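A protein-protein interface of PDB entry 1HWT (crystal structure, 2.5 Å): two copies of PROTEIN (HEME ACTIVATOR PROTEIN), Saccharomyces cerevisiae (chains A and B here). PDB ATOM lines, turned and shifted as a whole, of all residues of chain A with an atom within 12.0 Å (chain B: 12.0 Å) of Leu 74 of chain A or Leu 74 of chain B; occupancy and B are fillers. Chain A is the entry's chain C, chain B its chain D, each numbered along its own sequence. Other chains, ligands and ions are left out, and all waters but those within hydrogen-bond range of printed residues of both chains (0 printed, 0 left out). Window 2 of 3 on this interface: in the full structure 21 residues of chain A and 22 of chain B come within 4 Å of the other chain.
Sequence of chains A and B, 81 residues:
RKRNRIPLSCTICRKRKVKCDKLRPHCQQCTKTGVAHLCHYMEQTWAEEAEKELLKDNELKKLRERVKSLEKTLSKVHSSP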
ATOM      1  N   GLU A  65     -19.502  -3.569   8.812  1.00  0.00           N
ATOM      2  CA  GLU A  65     -20.106  -2.273   8.509  1.00  0.00           C
ATOM      3  C   GLU A  65     -21.571  -2.436   8.164  1.00  0.00           C
ATOM      4  O   GLU A  65     -22.395  -1.603   8.497  1.00  0.00           O
ATOM      5  CB  GLU A  65     -19.406  -1.618   7.326  1.00  0.00           C
ATOM      6  CG  GLU A  65     -18.178  -0.825   7.670  1.00  0.00           C
ATOM      7  CD  GLU A  65     -17.381  -0.454   6.436  1.00  0.00           C
ATOM      8  OE1 GLU A  65     -17.868  -0.722   5.323  1.00  0.00           O
ATOM      9  OE2 GLU A  65     -16.269   0.104   6.565  1.00  0.00           O
ATOM     10  N   ARG A  66     -21.893  -3.520   7.481  1.00  0.00           N
ATOM     11  CA  ARG A  66     -23.267  -3.772   7.083  1.00  0.00           C
ATOM     12  C   ARG A  66     -24.118  -4.182   8.279  1.00  0.00           C
ATOM     13  O   ARG A  66     -25.296  -3.834   8.362  1.00  0.00           O
ATOM     14  CB  ARG A  66     -23.310  -4.860   6.000  1.00  0.00           C
ATOM     15  CG  ARG A  66     -24.722  -5.332   5.634  1.00  0.00           C
ATOM     16  CD  ARG A  66     -25.381  -4.433   4.588  1.00  0.00           C
ATOM     17  NE  ARG A  66     -26.657  -4.987   4.119  1.00  0.00           N
ATOM     18  CZ  ARG A  66     -27.785  -4.284   3.960  1.00  0.00           C
ATOM     19  NH1 ARG A  66     -27.799  -2.982   4.230  1.00  0.00           N
ATOM     20  NH2 ARG A  66     -28.911  -4.885   3.554  1.00  0.00           N
ATOM     21  N   VAL A  67     -23.528  -4.923   9.207  1.00  0.00           N
ATOM     22  CA  VAL A  67     -24.276  -5.350  10.383  1.00  0.00           C
ATOM     23  C   VAL A  67     -24.596  -4.129  11.239  1.00  0.00           C
ATOM     24  O   VAL A  67     -25.683  -4.020  11.788  1.00  0.00           O
ATOM     25  CB  VAL A  67     -23.487  -6.375  11.216  1.00  0.00           C
ATOM     26  CG1 VAL A  67     -24.134  -6.564  12.562  1.00  0.00           C
ATOM     27  CG2 VAL A  67     -23.445  -7.707  10.478  1.00  0.00           C
ATOM     28  N   LYS A  68     -23.641  -3.211  11.351  1.00  0.00           N
ATOM     29  CA  LYS A  68     -23.865  -1.999  12.129  1.00  0.00           C
ATOM     30  C   LYS A  68     -25.027  -1.260  11.466  1.00  0.00           C
ATOM     31  O   LYS A  68     -26.029  -0.947  12.110  1.00  0.00           O
ATOM     32  CB  LYS A  68     -22.605  -1.122  12.134  1.00  0.00           C
ATOM     33  CG  LYS A  68     -21.627  -1.398  13.303  1.00  0.00           C
ATOM     34  CD  LYS A  68     -21.623  -2.884  13.777  1.00  0.00           C
ATOM     35  CE  LYS A  68     -21.645  -3.002  15.331  1.00  0.00           C
ATOM     36  NZ  LYS A  68     -22.011  -4.362  15.870  1.00  0.00           N
ATOM     37  N   SER A  69     -24.896  -1.008  10.167  1.00  0.00           N
ATOM     38  CA  SER A  69     -25.938  -0.326   9.421  1.00  0.00           C
ATOM     39  C   SER A  69     -27.276  -1.010   9.670  1.00  0.00           C
ATOM     40  O   SER A  69     -28.233  -0.373  10.115  1.00  0.00           O
ATOM     41  CB  SER A  69     -25.621  -0.344   7.925  1.00  0.00           C
ATOM     42  OG  SER A  69     -26.220   0.745   7.225  1.00  0.00           O
ATOM     43  N   LEU A  70     -27.352  -2.307   9.397  1.00  0.00           N
ATOM     44  CA  LEU A  70     -28.599  -3.040   9.598  1.00  0.00           C
ATOM     45  C   LEU A  70     -29.189  -2.922  11.014  1.00  0.00           C
ATOM     46  O   LEU A  70     -30.299  -2.410  11.197  1.00  0.00           O
ATOM     47  CB  LEU A  70     -28.404  -4.515   9.247  1.00  0.00           C
ATOM     48  CG  LEU A  70     -28.603  -4.925   7.783  1.00  0.00           C
ATOM     49  CD1 LEU A  70     -28.018  -6.321   7.562  1.00  0.00           C
ATOM     50  CD2 LEU A  70     -30.081  -4.908   7.441  1.00  0.00           C
ATOM     51  N   GLU A  71     -28.464  -3.390  12.025  1.00  0.00           N
ATOM     52  CA  GLU A  71     -28.990  -3.335  13.397  1.00  0.00           C
ATOM     53  C   GLU A  71     -29.205  -1.901  13.899  1.00  0.00           C
ATOM     54  O   GLU A  71     -30.215  -1.601  14.564  1.00  0.00           O
ATOM     55  CB  GLU A  71     -28.057  -4.083  14.351  1.00  0.00           C
ATOM     56  CG  GLU A  71     -26.715  -3.411  14.528  1.00  0.00           C
ATOM     57  CD  GLU A  71     -25.658  -4.361  15.052  1.00  0.00           C
ATOM     58  OE1 GLU A  71     -25.963  -5.570  15.180  1.00  0.00           O
ATOM     59  OE2 GLU A  71     -24.529  -3.897  15.334  1.00  0.00           O
ATOM     60  N   LYS A  72     -28.259  -1.022  13.570  1.00  0.00           N
ATOM     61  CA  LYS A  72     -28.337   0.381  13.977  1.00  0.00           C
ATOM     62  C   LYS A  72     -29.375   1.121  13.147  1.00  0.00           C
ATOM     63  O   LYS A  72     -29.339   2.353  13.030  1.00  0.00           O
ATOM     64  CB  LYS A  72     -26.971   1.054  13.832  1.00  0.00           C
ATOM     65  CG  LYS A  72     -26.057   0.887  15.064  1.00  0.00           C
ATOM     66  CD  LYS A  72     -25.056  -0.261  14.877  1.00  0.00           C
ATOM     67  CE  LYS A  72     -24.506  -0.782  16.218  1.00  0.00           C
ATOM     68  NZ  LYS A  72     -23.497   0.171  16.764  1.00  0.00           N
ATOM     69  N   THR A  73     -30.272   0.341  12.550  1.00  0.00           N
ATOM     70  CA  THR A  73     -31.369   0.856  11.742  1.00  0.00           C
ATOM     71  C   THR A  73     -32.594   0.111  12.247  1.00  0.00           C
ATOM     72  O   THR A  73     -33.723   0.544  12.033  1.00  0.00           O
ATOM     73  CB  THR A  73     -31.168   0.583  10.213  1.00  0.00           C
ATOM     74  OG1 THR A  73     -31.001   1.834   9.530  1.00  0.00           O
ATOM     75  CG2 THR A  73     -32.381  -0.154   9.606  1.00  0.00           C
ATOM     76  N   LEU A  74     -32.376  -1.019  12.913  1.00  0.00           N
ATOM     77  CA  LEU A  74     -33.508  -1.756  13.451  1.00  0.00           C
ATOM     78  C   LEU A  74     -34.024  -1.007  14.670  1.00  0.00           C
ATOM     79  O   LEU A  74     -34.851  -1.604  15.401  1.00  0.00           O
ATOM     80  CB  LEU A  74     -33.117  -3.174  13.871  1.00  0.00           C
ATOM     81  CG  LEU A  74     -33.971  -4.281  13.232  1.00  0.00           C
ATOM     82  CD1 LEU A  74     -33.031  -5.283  12.585  1.00  0.00           C
ATOM     83  CD2 LEU A  74     -34.871  -4.979  14.256  1.00  0.00           C
ATOM     84  N   ARG B  64     -22.150 -13.250   8.415  1.00  0.00           N
ATOM     85  CA  ARG B  64     -23.086 -13.436   7.303  1.00  0.00           C
ATOM     86  C   ARG B  64     -24.434 -13.997   7.786  1.00  0.00           C
ATOM     87  O   ARG B  64     -25.489 -13.627   7.274  1.00  0.00           O
ATOM     88  CB  ARG B  64     -22.482 -14.369   6.244  1.00  0.00           C
ATOM     89  CG  ARG B  64     -21.291 -13.773   5.500  1.00  0.00           C
ATOM     90  CD  ARG B  64     -20.918 -14.580   4.278  1.00  0.00           C
ATOM     91  NE  ARG B  64     -19.789 -15.475   4.513  1.00  0.00           N
ATOM     92  CZ  ARG B  64     -18.631 -15.422   3.853  1.00  0.00           C
ATOM     93  NH1 ARG B  64     -18.451 -14.501   2.909  1.00  0.00           N
ATOM     94  NH2 ARG B  64     -17.660 -16.298   4.144  1.00  0.00           N
ATOM     95  N   GLU B  65     -24.398 -14.897   8.767  1.00  0.00           N
ATOM     96  CA  GLU B  65     -25.632 -15.461   9.293  1.00  0.00           C
ATOM     97  C   GLU B  65     -26.365 -14.309   9.960  1.00  0.00           C
ATOM     98  O   GLU B  65     -27.590 -14.283  10.030  1.00  0.00           O
ATOM     99  CB  GLU B  65     -25.342 -16.532  10.347  1.00  0.00           C
ATOM    100  CG  GLU B  65     -24.867 -17.883   9.835  1.00  0.00           C
ATOM    101  CD  GLU B  65     -24.354 -18.746  10.973  1.00  0.00           C
ATOM    102  OE1 GLU B  65     -24.684 -18.431  12.141  1.00  0.00           O
ATOM    103  OE2 GLU B  65     -23.622 -19.731  10.716  1.00  0.00           O
ATOM    104  N   ARG B  66     -25.583 -13.362  10.462  1.00  0.00           N
ATOM    105  CA  ARG B  66     -26.106 -12.197  11.158  1.00  0.00           C
ATOM    106  C   ARG B  66     -26.747 -11.189  10.223  1.00  0.00           C
ATOM    107  O   ARG B  66     -27.785 -10.602  10.542  1.00  0.00           O
ATOM    108  CB  ARG B  66     -24.986 -11.518  11.943  1.00  0.00           C
ATOM    109  CG  ARG B  66     -25.457 -10.346  12.790  1.00  0.00           C
ATOM    110  CD  ARG B  66     -25.713 -10.751  14.248  1.00  0.00           C
ATOM    111  NE  ARG B  66     -26.230  -9.613  14.999  1.00  0.00           N
ATOM    112  CZ  ARG B  66     -27.457  -9.553  15.490  1.00  0.00           C
ATOM    113  NH1 ARG B  66     -28.279 -10.578  15.305  1.00  0.00           N
ATOM    114  NH2 ARG B  66     -27.870  -8.463  16.126  1.00  0.00           N
ATOM    115  N   VAL B  67     -26.121 -10.972   9.074  1.00  0.00           N
ATOM    116  CA  VAL B  67     -26.670 -10.044   8.098  1.00  0.00           C
ATOM    117  C   VAL B  67     -27.997 -10.644   7.623  1.00  0.00           C
ATOM    118  O   VAL B  67     -29.025  -9.956   7.547  1.00  0.00           O
ATOM    119  CB  VAL B  67     -25.713  -9.874   6.900  1.00  0.00           C
ATOM    120  CG1 VAL B  67     -26.412  -9.121   5.784  1.00  0.00           C
ATOM    121  CG2 VAL B  67     -24.464  -9.131   7.338  1.00  0.00           C
ATOM    122  N   LYS B  68     -27.970 -11.942   7.328  1.00  0.00           N
ATOM    123  CA  LYS B  68     -29.162 -12.650   6.881  1.00  0.00           C
ATOM    124  C   LYS B  68     -30.240 -12.611   7.965  1.00  0.00           C
ATOM    125  O   LYS B  68     -31.419 -12.416   7.670  1.00  0.00           O
ATOM    126  CB  LYS B  68     -28.821 -14.104   6.546  1.00  0.00           C
ATOM    127  CG  LYS B  68     -30.025 -15.006   6.344  1.00  0.00           C
ATOM    128  CD  LYS B  68     -29.623 -16.333   5.671  1.00  0.00           C
ATOM    129  CE  LYS B  68     -30.202 -16.413   4.251  1.00  0.00           C
ATOM    130  NZ  LYS B  68     -29.958 -17.723   3.555  1.00  0.00           N
ATOM    131  N   SER B  69     -29.841 -12.781   9.223  1.00  0.00           N
ATOM    132  CA  SER B  69     -30.803 -12.775  10.318  1.00  0.00           C
ATOM    133  C   SER B  69     -31.398 -11.403  10.549  1.00  0.00           C
ATOM    134  O   SER B  69     -32.593 -11.268  10.778  1.00  0.00           O
ATOM    135  CB  SER B  69     -30.154 -13.254  11.611  1.00  0.00           C
ATOM    136  OG  SER B  69     -31.082 -13.184  12.679  1.00  0.00           O
ATOM    137  N   LEU B  70     -30.563 -10.381  10.512  1.00  0.00           N
ATOM    138  CA  LEU B  70     -31.050  -9.040  10.739  1.00  0.00           C
ATOM    139  C   LEU B  70     -32.011  -8.688   9.626  1.00  0.00           C
ATOM    140  O   LEU B  70     -33.148  -8.318   9.895  1.00  0.00           O
ATOM    141  CB  LEU B  70     -29.887  -8.053  10.772  1.00  0.00           C
ATOM    142  CG  LEU B  70     -29.213  -7.774  12.118  1.00  0.00           C
ATOM    143  CD1 LEU B  70     -27.837  -7.225  11.842  1.00  0.00           C
ATOM    144  CD2 LEU B  70     -30.016  -6.783  12.938  1.00  0.00           C
ATOM    145  N   GLU B  71     -31.544  -8.806   8.379  1.00  0.00           N
ATOM    146  CA  GLU B  71     -32.365  -8.510   7.189  1.00  0.00           C
ATOM    147  C   GLU B  71     -33.674  -9.315   7.315  1.00  0.00           C
ATOM    148  O   GLU B  71     -34.776  -8.759   7.237  1.00  0.00           O
ATOM    149  CB  GLU B  71     -31.613  -8.920   5.893  1.00  0.00           C
ATOM    150  CG  GLU B  71     -30.732  -7.799   5.235  1.00  0.00           C
ATOM    151  CD  GLU B  71     -29.815  -8.307   4.093  1.00  0.00           C
ATOM    152  OE1 GLU B  71     -29.917  -9.504   3.712  1.00  0.00           O
ATOM    153  OE2 GLU B  71     -28.987  -7.504   3.581  1.00  0.00           O
ATOM    154  N   LYS B  72     -33.534 -10.624   7.534  1.00  0.00           N
ATOM    155  CA  LYS B  72     -34.670 -11.527   7.686  1.00  0.00           C
ATOM    156  C   LYS B  72     -35.426 -11.207   8.970  1.00  0.00           C
ATOM    157  O   LYS B  72     -36.045 -12.094   9.564  1.00  0.00           O
ATOM    158  CB  LYS B  72     -34.185 -12.986   7.739  1.00  0.00           C
ATOM    159  CG  LYS B  72     -34.404 -13.794   6.452  1.00  0.00           C
ATOM    160  CD  LYS B  72     -33.204 -13.706   5.508  1.00  0.00           C
ATOM    161  CE  LYS B  72     -33.253 -12.463   4.600  1.00  0.00           C
ATOM    162  NZ  LYS B  72     -31.935 -12.197   3.900  1.00  0.00           N
ATOM    163  N   THR B  73     -35.349  -9.950   9.408  1.00  0.00           N
ATOM    164  CA  THR B  73     -36.019  -9.510  10.622  1.00  0.00           C
ATOM    165  C   THR B  73     -36.740  -8.186  10.408  1.00  0.00           C
ATOM    166  O   THR B  73     -37.932  -8.069  10.714  1.00  0.00           O
ATOM    167  CB  THR B  73     -35.015  -9.363  11.803  1.00  0.00           C
ATOM    168  OG1 THR B  73     -35.262 -10.395  12.768  1.00  0.00           O
ATOM    169  CG2 THR B  73     -35.162  -8.016  12.487  1.00  0.00           C
ATOM    170  N   LEU B  74     -36.043  -7.180   9.893  1.00  0.00           N
ATOM    171  CA  LEU B  74     -36.711  -5.897   9.688  1.00  0.00           C
ATOM    172  C   LEU B  74     -37.372  -5.775   8.300  1.00  0.00           C
ATOM    173  O   LEU B  74     -37.421  -4.639   7.751  1.00  0.00           O
ATOM    174  CB  LEU B  74     -35.734  -4.734   9.931  1.00  0.00           C
ATOM    175  CG  LEU B  74     -34.822  -4.339   8.777  1.00  0.00           C
ATOM    176  CD1 LEU B  74     -34.143  -2.984   9.049  1.00  0.00           C
ATOM    177  CD2 LEU B  74     -33.797  -5.440   8.598  1.00  0.00           C
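NH2 of Arg 66 of chain A lies within salt-bridge range of OE2 of Glu 71 of chain B, at 2.6 Å. The side-chain carboxylate of Glu 71 of chain A lies within salt-bridge range of the guanidinium group of Arg 66 of chain B (3.6 Å).
The side-chain amino group (NZ) of Lys 68 of chain A is in salt-bridge range of the side-chain carboxylate (OE2) of Glu 71 of chain A (2.6 Å). The backbone carbonyl oxygen (O) of Ser 69 of chain B lies close to the side-chain hydroxyl (OG1) of Thr 73 of chain B (3.4 Å). NZ of Lys 72 of chain B is in salt-bridge range of OE1 of Glu 71 of chain B (3.4 Å).
Among the printed residues, pairs that only touch across the chains: Val 67 of chain A with Val 67 of chain B (3.6 Å), Val 67 of chain A with Leu 70 of chain B (3.8 Å), Leu 70 of chain A with Val 67 of chain B (3.7 Å), Leu 70 of chain A with Leu 70 of chain B (3.8 Å), Leu 70 of chain A with Glu 71 of chain B (3.7 Å), Leu 70 of chain A with Leu 74 of chain B (3.9 Å), Glu 71 of chain A with Leu 70 of chain B (3.6 Å), Thr 73 of chain A with Leu 74 of chain B (3.4 Å), Leu 74 of chain A with Leu 70 of chain B (3.4 Å), Leu 74 of chain A with Thr 73 of chain B (3.5 Å) and Leu 74 of chain A with Leu 74 of chain B (3.8 Å).
Glu 65 of chain A touches none of the printed residues of chain B. Printed residues of chain B within 4 Å of Arg 66 of chain A: Glu 71 (2.6 Å). Printed residues of chain B within 4 Å of Val 67 of chain A: Val 67 and Leu 70. Lys 68 of chain A touches none of the printed residues of chain B. Printed residues of chain B within 4 Å of Leu 70 of chain A: Val 67, Leu 70, Glu 71 and Leu 74. Printed residues of chain B within 4 Å of Thr 73 of chain A: Leu 74 (3.4 Å). Leu 74 of chain A touches just these residues of chain B: Leu 70 (3.4 Å), Thr 73 (3.5 Å) and Leu 74 (3.8 Å). Of the printed residues of chain A, Val 67 of chain B touches Val 67 (3.6 Å) and Leu 70 (3.7 Å). Leu 70 of chain B touches four residues of chain A. Thr 73 of chain B touches one residue of chain A. Of chain A, only Leu 70 (3.9 Å), Thr 73 (3.4 Å) and Leu 74 (3.8 Å) come within 4 Å of Leu 74 of chain B. The nearest residue of chain B that does not touch Leu 74 of chain A is Glu 71 of chain B (5.7 Å).
Arg 66 of chain A touches Glu 71 of chain B, and with the chains exchanged Glu 71 of chain A touches Arg 66 of chain B. Val 67 of chain B touches its own counterpart, Val 67 of chain A. Leu 70 of chain A touches Glu 71 of chain B, and with the chains exchanged Glu 71 of chain A touches Leu 70 of chain B. Leu 70 of chain A touches Leu 74 of chain B, and with the chains exchanged Leu 74 of chain A touches Leu 70 of chain B. Positions printed for both chains: 65, 66, 67, 68, 69, 70, 71, 72, 73 and 74.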
